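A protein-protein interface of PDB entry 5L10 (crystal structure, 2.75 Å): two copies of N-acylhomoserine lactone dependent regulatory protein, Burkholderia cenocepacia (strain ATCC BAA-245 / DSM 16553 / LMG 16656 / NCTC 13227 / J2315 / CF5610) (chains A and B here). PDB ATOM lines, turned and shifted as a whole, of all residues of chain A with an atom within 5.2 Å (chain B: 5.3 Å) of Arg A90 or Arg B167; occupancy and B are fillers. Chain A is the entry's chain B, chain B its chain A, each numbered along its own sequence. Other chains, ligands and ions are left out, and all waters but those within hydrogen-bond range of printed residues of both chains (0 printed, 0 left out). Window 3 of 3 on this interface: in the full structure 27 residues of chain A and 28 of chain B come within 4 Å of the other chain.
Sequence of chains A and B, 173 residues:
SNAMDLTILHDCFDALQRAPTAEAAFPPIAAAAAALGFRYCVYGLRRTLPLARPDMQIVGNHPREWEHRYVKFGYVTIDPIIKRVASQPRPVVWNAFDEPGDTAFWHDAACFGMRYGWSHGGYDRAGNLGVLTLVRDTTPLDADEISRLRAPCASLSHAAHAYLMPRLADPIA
Of the 16 printed residues of chain B, 4 touch a printed residue of chain A. Hydrophobic or aromatic side chains of chain B within 4 Å of the printed part of chain A: Ala B162, Tyr B163 and Pro B166. Of the 8 printed residues of chain A, 2 touch a printed residue of chain B. Printed residues of chain A that touch a printed residue of chain B: Pro A89 and Arg A90. Among the printed residues, 6 pairs touch across the chains.
Printed residues of chain B within 4 Å of Arg A90: Ala B162, Tyr B163, Pro B166 and Arg B167. Printed residues of chain A within 4 Å of Arg B167: Arg A90. Of the printed residues of chain A, Tyr B163 touches Arg A90 (3.6 Å). Printed residues of chain A within 4 Å of Pro B166: Pro A89 and Arg A90. Printed residues of chain B within 4 Å of Pro A89: Ala B162 (3.3 Å) and Pro B166 (3.5 Å). Of the printed residues of chain A, Ala B162 touches Pro A89 (3.3 Å) and Arg A90 (2.7 Å). Val A85 touches none of the printed residues of chain B. Ala B19 touches none of the printed residues of chain A. The nearest printed residue of chain A that does not touch Arg B167 is Pro A89 (6.7 Å).
No position is printed for both chains.
The backbone carbonyl oxygen (O) of Ala B162 is in hydrogen-bond range of the guanidinium group (NH1) of Arg A90, at 2.7 Å. The guanidinium group (NH1) of Arg A90 sits close to the guanidinium group (NH1) of Arg B167, at 3.0 Å.
NH2 of Arg B167 is in hydrogen-bond range of O of Ala B19 (3.2 Å). The guanidinium group (NH2) of Arg B167 is in hydrogen-bond range of the backbone carbonyl oxygen (O) of Tyr B163 (2.5 Å). O of Arg A90 sits at hydrogen-bond distance from NE2 of Gln A88 (2.5 Å). A ring nitrogen (ND1) of His A120 sits close to the backbone carbonyl oxygen (O) of Pro A89 (3.4 Å).
Among the printed residues, merely in contact across the chains: Pro A89 with Ala B162 (3.3 Å), Pro A89 with Pro B166 (3.5 Å), Arg A90 with Tyr B163 (3.6 Å) and Arg A90 with Pro B166 (3.9 Å).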
ATOM      1  N   VAL A  85      13.589   5.665  27.093  1.00  0.00           N
ATOM      2  CA  VAL A  85      14.382   5.775  28.315  1.00  0.00           C
ATOM      3  C   VAL A  85      15.552   4.810  28.329  1.00  0.00           C
ATOM      4  O   VAL A  85      16.447   4.945  29.170  1.00  0.00           O
ATOM      5  CB  VAL A  85      13.524   5.549  29.575  1.00  0.00           C
ATOM      6  CG1 VAL A  85      12.364   6.527  29.598  1.00  0.00           C
ATOM      7  CG2 VAL A  85      13.033   4.116  29.645  1.00  0.00           C
ATOM      8  N   GLN A  88      18.679   6.534  26.141  1.00  0.00           N
ATOM      9  CA  GLN A  88      18.984   7.879  26.611  1.00  0.00           C
ATOM     10  C   GLN A  88      18.899   7.895  28.129  1.00  0.00           C
ATOM     11  O   GLN A  88      18.008   7.258  28.705  1.00  0.00           O
ATOM     12  CB  GLN A  88      18.010   8.904  26.009  1.00  0.00           C
ATOM     13  CG  GLN A  88      17.937  10.237  26.735  1.00  0.00           C
ATOM     14  CD  GLN A  88      16.550  10.846  26.683  1.00  0.00           C
ATOM     15  OE1 GLN A  88      16.281  11.747  25.887  1.00  0.00           O
ATOM     16  NE2 GLN A  88      15.663  10.360  27.540  1.00  0.00           N
ATOM     17  N   PRO A  89      19.801   8.606  28.801  1.00  0.00           N
ATOM     18  CA  PRO A  89      19.765   8.674  30.272  1.00  0.00           C
ATOM     19  C   PRO A  89      18.940   9.817  30.860  1.00  0.00           C
ATOM     20  O   PRO A  89      18.768   9.842  32.082  1.00  0.00           O
ATOM     21  CB  PRO A  89      21.250   8.848  30.621  1.00  0.00           C
ATOM     22  CG  PRO A  89      21.910   9.400  29.369  1.00  0.00           C
ATOM     23  CD  PRO A  89      20.934   9.364  28.241  1.00  0.00           C
ATOM     24  N   ARG A  90      18.426  10.746  30.049  1.00  0.00           N
ATOM     25  CA  ARG A  90      17.606  11.839  30.551  1.00  0.00           C
ATOM     26  C   ARG A  90      16.147  11.414  30.672  1.00  0.00           C
ATOM     27  O   ARG A  90      15.701  10.474  30.006  1.00  0.00           O
ATOM     28  CB  ARG A  90      17.727  13.053  29.630  1.00  0.00           C
ATOM     29  CG  ARG A  90      18.798  14.046  30.064  1.00  0.00           C
ATOM     30  CD  ARG A  90      19.194  14.991  28.935  1.00  0.00           C
ATOM     31  NE  ARG A  90      19.735  14.275  27.783  1.00  0.00           N
ATOM     32  CZ  ARG A  90      20.977  13.805  27.708  1.00  0.00           C
ATOM     33  NH1 ARG A  90      21.814  13.966  28.723  1.00  0.00           N
ATOM     34  NH2 ARG A  90      21.380  13.166  26.618  1.00  0.00           N
ATOM     35  N   PRO A  91      15.374  12.080  31.529  1.00  0.00           N
ATOM     36  CA  PRO A  91      13.949  11.742  31.647  1.00  0.00           C
ATOM     37  C   PRO A  91      13.172  12.041  30.372  1.00  0.00           C
ATOM     38  O   PRO A  91      13.577  12.849  29.532  1.00  0.00           O
ATOM     39  CB  PRO A  91      13.467  12.628  32.803  1.00  0.00           C
ATOM     40  CG  PRO A  91      14.706  12.963  33.572  1.00  0.00           C
ATOM     41  CD  PRO A  91      15.797  13.051  32.553  1.00  0.00           C
ATOM     42  N   VAL A  92      12.027  11.375  30.245  1.00  0.00           N
ATOM     43  CA  VAL A  92      11.142  11.497  29.091  1.00  0.00           C
ATOM     44  C   VAL A  92       9.767  11.930  29.581  1.00  0.00           C
ATOM     45  O   VAL A  92       9.199  11.303  30.483  1.00  0.00           O
ATOM     46  CB  VAL A  92      11.051  10.173  28.308  1.00  0.00           C
ATOM     47  CG1 VAL A  92      10.033  10.276  27.179  1.00  0.00           C
ATOM     48  CG2 VAL A  92      12.413   9.788  27.763  1.00  0.00           C
ATOM     49  N   SER A 119       8.758   9.698  32.835  1.00  0.00           N
ATOM     50  CA  SER A 119       9.436   8.410  32.894  1.00  0.00           C
ATOM     51  C   SER A 119      10.945   8.581  32.846  1.00  0.00           C
ATOM     52  O   SER A 119      11.467   9.414  32.098  1.00  0.00           O
ATOM     53  CB  SER A 119       8.989   7.498  31.749  1.00  0.00           C
ATOM     54  OG  SER A 119       7.639   7.103  31.912  1.00  0.00           O
ATOM     55  N   HIS A 120      11.641   7.769  33.638  1.00  0.00           N
ATOM     56  CA  HIS A 120      13.093   7.775  33.655  1.00  0.00           C
ATOM     57  C   HIS A 120      13.592   6.359  33.895  1.00  0.00           C
ATOM     58  O   HIS A 120      13.062   5.643  34.750  1.00  0.00           O
ATOM     59  CB  HIS A 120      13.642   8.715  34.728  1.00  0.00           C
ATOM     60  CG  HIS A 120      15.129   8.658  34.862  1.00  0.00           C
ATOM     61  ND1 HIS A 120      15.982   9.297  33.988  1.00  0.00           N
ATOM     62  CD2 HIS A 120      15.918   8.015  35.755  1.00  0.00           C
ATOM     63  CE1 HIS A 120      17.231   9.061  34.343  1.00  0.00           C
ATOM     64  NE2 HIS A 120      17.219   8.285  35.412  1.00  0.00           N
ATOM     65  N   LEU B  16      21.508  22.720  33.541  1.00  0.00           N
ATOM     66  CA  LEU B  16      21.807  21.468  32.859  1.00  0.00           C
ATOM     67  C   LEU B  16      20.983  21.285  31.593  1.00  0.00           C
ATOM     68  O   LEU B  16      21.335  20.444  30.761  1.00  0.00           O
ATOM     69  CB  LEU B  16      21.585  20.287  33.806  1.00  0.00           C
ATOM     70  CG  LEU B  16      22.567  20.188  34.977  1.00  0.00           C
ATOM     71  CD1 LEU B  16      22.270  18.971  35.828  1.00  0.00           C
ATOM     72  CD2 LEU B  16      23.999  20.156  34.477  1.00  0.00           C
ATOM     73  N   ALA B  19      23.297  22.797  28.719  1.00  0.00           N
ATOM     74  CA  ALA B  19      24.667  22.297  28.810  1.00  0.00           C
ATOM     75  C   ALA B  19      24.797  21.104  27.877  1.00  0.00           C
ATOM     76  O   ALA B  19      24.561  19.956  28.285  1.00  0.00           O
ATOM     77  CB  ALA B  19      25.026  21.916  30.244  1.00  0.00           C
ATOM     78  N   PRO B  20      25.173  21.324  26.617  1.00  0.00           N
ATOM     79  CA  PRO B  20      25.278  20.212  25.668  1.00  0.00           C
ATOM     80  C   PRO B  20      26.605  19.471  25.718  1.00  0.00           C
ATOM     81  O   PRO B  20      26.810  18.554  24.916  1.00  0.00           O
ATOM     82  CB  PRO B  20      25.091  20.910  24.312  1.00  0.00           C
ATOM     83  CG  PRO B  20      25.479  22.364  24.549  1.00  0.00           C
ATOM     84  CD  PRO B  20      25.632  22.594  26.033  1.00  0.00           C
ATOM     85  N   THR B  21      27.508  19.840  26.623  1.00  0.00           N
ATOM     86  CA  THR B  21      28.821  19.222  26.729  1.00  0.00           C
ATOM     87  C   THR B  21      29.126  18.928  28.191  1.00  0.00           C
ATOM     88  O   THR B  21      28.498  19.477  29.100  1.00  0.00           O
ATOM     89  CB  THR B  21      29.920  20.121  26.151  1.00  0.00           C
ATOM     90  OG1 THR B  21      29.992  21.330  26.917  1.00  0.00           O
ATOM     91  CG2 THR B  21      29.623  20.469  24.705  1.00  0.00           C
ATOM     92  N   ALA B  22      30.109  18.050  28.411  1.00  0.00           N
ATOM     93  CA  ALA B  22      30.542  17.762  29.776  1.00  0.00           C
ATOM     94  C   ALA B  22      31.251  18.957  30.398  1.00  0.00           C
ATOM     95  O   ALA B  22      31.251  19.113  31.624  1.00  0.00           O
ATOM     96  CB  ALA B  22      31.455  16.536  29.793  1.00  0.00           C
ATOM     97  N   ALA B  25      28.368  21.000  31.612  1.00  0.00           N
ATOM     98  CA  ALA B  25      27.505  20.307  32.558  1.00  0.00           C
ATOM     99  C   ALA B  25      28.123  20.171  33.938  1.00  0.00           C
ATOM    100  O   ALA B  25      27.385  20.028  34.920  1.00  0.00           O
ATOM    101  CB  ALA B  25      27.147  18.914  32.040  1.00  0.00           C
ATOM    102  N   ALA B 162      22.783  11.514  34.434  1.00  0.00           N
ATOM    103  CA  ALA B 162      21.932  11.780  33.282  1.00  0.00           C
ATOM    104  C   ALA B 162      22.478  12.873  32.375  1.00  0.00           C
ATOM    105  O   ALA B 162      22.233  12.837  31.163  1.00  0.00           O
ATOM    106  CB  ALA B 162      20.522  12.161  33.740  1.00  0.00           C
ATOM    107  N   TYR B 163      23.217  13.838  32.923  1.00  0.00           N
ATOM    108  CA  TYR B 163      23.666  14.983  32.145  1.00  0.00           C
ATOM    109  C   TYR B 163      25.174  15.059  31.952  1.00  0.00           C
ATOM    110  O   TYR B 163      25.618  15.685  30.986  1.00  0.00           O
ATOM    111  CB  TYR B 163      23.190  16.290  32.795  1.00  0.00           C
ATOM    112  CG  TYR B 163      21.688  16.447  32.819  1.00  0.00           C
ATOM    113  CD1 TYR B 163      21.020  17.066  31.769  1.00  0.00           C
ATOM    114  CD2 TYR B 163      20.939  15.979  33.889  1.00  0.00           C
ATOM    115  CE1 TYR B 163      19.645  17.215  31.787  1.00  0.00           C
ATOM    116  CE2 TYR B 163      19.564  16.123  33.914  1.00  0.00           C
ATOM    117  CZ  TYR B 163      18.923  16.742  32.863  1.00  0.00           C
ATOM    118  OH  TYR B 163      17.555  16.886  32.884  1.00  0.00           O
ATOM    119  N   LEU B 164      25.968  14.453  32.834  1.00  0.00           N
ATOM    120  CA  LEU B 164      27.422  14.513  32.728  1.00  0.00           C
ATOM    121  C   LEU B 164      28.020  13.232  32.157  1.00  0.00           C
ATOM    122  O   LEU B 164      28.773  13.285  31.180  1.00  0.00           O
ATOM    123  CB  LEU B 164      28.040  14.813  34.101  1.00  0.00           C
ATOM    124  CG  LEU B 164      29.556  14.984  34.108  1.00  0.00           C
ATOM    125  CD1 LEU B 164      29.945  16.104  33.171  1.00  0.00           C
ATOM    126  CD2 LEU B 164      30.054  15.268  35.508  1.00  0.00           C
ATOM    127  N   MET B 165      27.704  12.084  32.746  1.00  0.00           N
ATOM    128  CA  MET B 165      28.238  10.808  32.280  1.00  0.00           C
ATOM    129  C   MET B 165      28.052  10.549  30.769  1.00  0.00           C
ATOM    130  O   MET B 165      29.026  10.216  30.089  1.00  0.00           O
ATOM    131  CB  MET B 165      27.625   9.657  33.091  1.00  0.00           C
ATOM    132  CG  MET B 165      27.732   8.307  32.406  1.00  0.00           C
ATOM    133  SD  MET B 165      27.492   6.768  33.581  1.00  0.00           S
ATOM    134  CE  MET B 165      25.745   7.178  34.317  1.00  0.00           C
ATOM    135  N   PRO B 166      26.833  10.705  30.231  1.00  0.00           N
ATOM    136  CA  PRO B 166      26.646  10.444  28.793  1.00  0.00           C
ATOM    137  C   PRO B 166      27.428  11.383  27.899  1.00  0.00           C
ATOM    138  O   PRO B 166      27.731  11.013  26.758  1.00  0.00           O
ATOM    139  CB  PRO B 166      25.136  10.626  28.596  1.00  0.00           C
ATOM    140  CG  PRO B 166      24.743  11.557  29.667  1.00  0.00           C
ATOM    141  CD  PRO B 166      25.572  11.161  30.846  1.00  0.00           C
ATOM    142  N   ARG B 167      27.753  12.586  28.369  1.00  0.00           N
ATOM    143  CA  ARG B 167      28.533  13.533  27.588  1.00  0.00           C
ATOM    144  C   ARG B 167      30.029  13.397  27.830  1.00  0.00           C
ATOM    145  O   ARG B 167      30.819  14.041  27.131  1.00  0.00           O
ATOM    146  CB  ARG B 167      28.062  14.958  27.887  1.00  0.00           C
ATOM    147  CG  ARG B 167      26.549  15.074  27.825  1.00  0.00           C
ATOM    148  CD  ARG B 167      26.086  16.429  27.344  1.00  0.00           C
ATOM    149  NE  ARG B 167      24.634  16.461  27.179  1.00  0.00           N
ATOM    150  CZ  ARG B 167      23.778  16.729  28.161  1.00  0.00           C
ATOM    151  NH1 ARG B 167      22.475  16.739  27.922  1.00  0.00           N
ATOM    152  NH2 ARG B 167      24.226  16.987  29.382  1.00  0.00           N
ATOM    153  N   LEU B 168      30.427  12.581  28.803  1.00  0.00           N
ATOM    154  CA  LEU B 168      31.799  12.107  28.908  1.00  0.00           C
ATOM    155  C   LEU B 168      32.016  10.850  28.076  1.00  0.00           C
ATOM    156  O   LEU B 168      33.036  10.727  27.387  1.00  0.00           O
ATOM    157  CB  LEU B 168      32.153  11.827  30.370  1.00  0.00           C
ATOM    158  CG  LEU B 168      32.300  13.039  31.287  1.00  0.00           C
ATOM    159  CD1 LEU B 168      32.363  12.595  32.734  1.00  0.00           C
ATOM    160  CD2 LEU B 168      33.544  13.823  30.916  1.00  0.00           C
ATOM    161  N   ALA B 169      31.064   9.918  28.119  1.00  0.00           N
ATOM    162  CA  ALA B 169      31.208   8.675  27.369  1.00  0.00           C
ATOM    163  C   ALA B 169      31.140   8.926  25.868  1.00  0.00           C
ATOM    164  O   ALA B 169      31.950   8.390  25.101  1.00  0.00           O
ATOM    165  CB  ALA B 169      30.131   7.678  27.798  1.00  0.00           C
ATOM    166  N   ASP B 170      30.177   9.737  25.429  1.00  0.00           N
ATOM    167  CA  ASP B 170      29.944  10.006  24.009  1.00  0.00           C
ATOM    168  C   ASP B 170      29.816  11.508  23.797  1.00  0.00           C
ATOM    169  O   ASP B 170      28.703  12.053  23.795  1.00  0.00           O
ATOM    170  CB  ASP B 170      28.690   9.288  23.510  1.00  0.00           C
ATOM    171  CG  ASP B 170      28.834   7.778  23.521  1.00  0.00           C
ATOM    172  OD1 ASP B 170      29.025   7.202  24.613  1.00  0.00           O
ATOM    173  OD2 ASP B 170      28.746   7.164  22.436  1.00  0.00           O
ATOM    174  N   PRO B 171      30.932  12.215  23.617  1.00  0.00           N
ATOM    175  CA  PRO B 171      30.846  13.654  23.340  1.00  0.00           C
ATOM    176  C   PRO B 171      30.165  13.913  22.005  1.00  0.00           C
ATOM    177  O   PRO B 171      30.264  13.118  21.069  1.00  0.00           O
ATOM    178  CB  PRO B 171      32.313  14.103  23.313  1.00  0.00           C
ATOM    179  CG  PRO B 171      33.072  13.024  24.011  1.00  0.00           C
ATOM    180  CD  PRO B 171      32.325  11.756  23.746  1.00  0.00           C
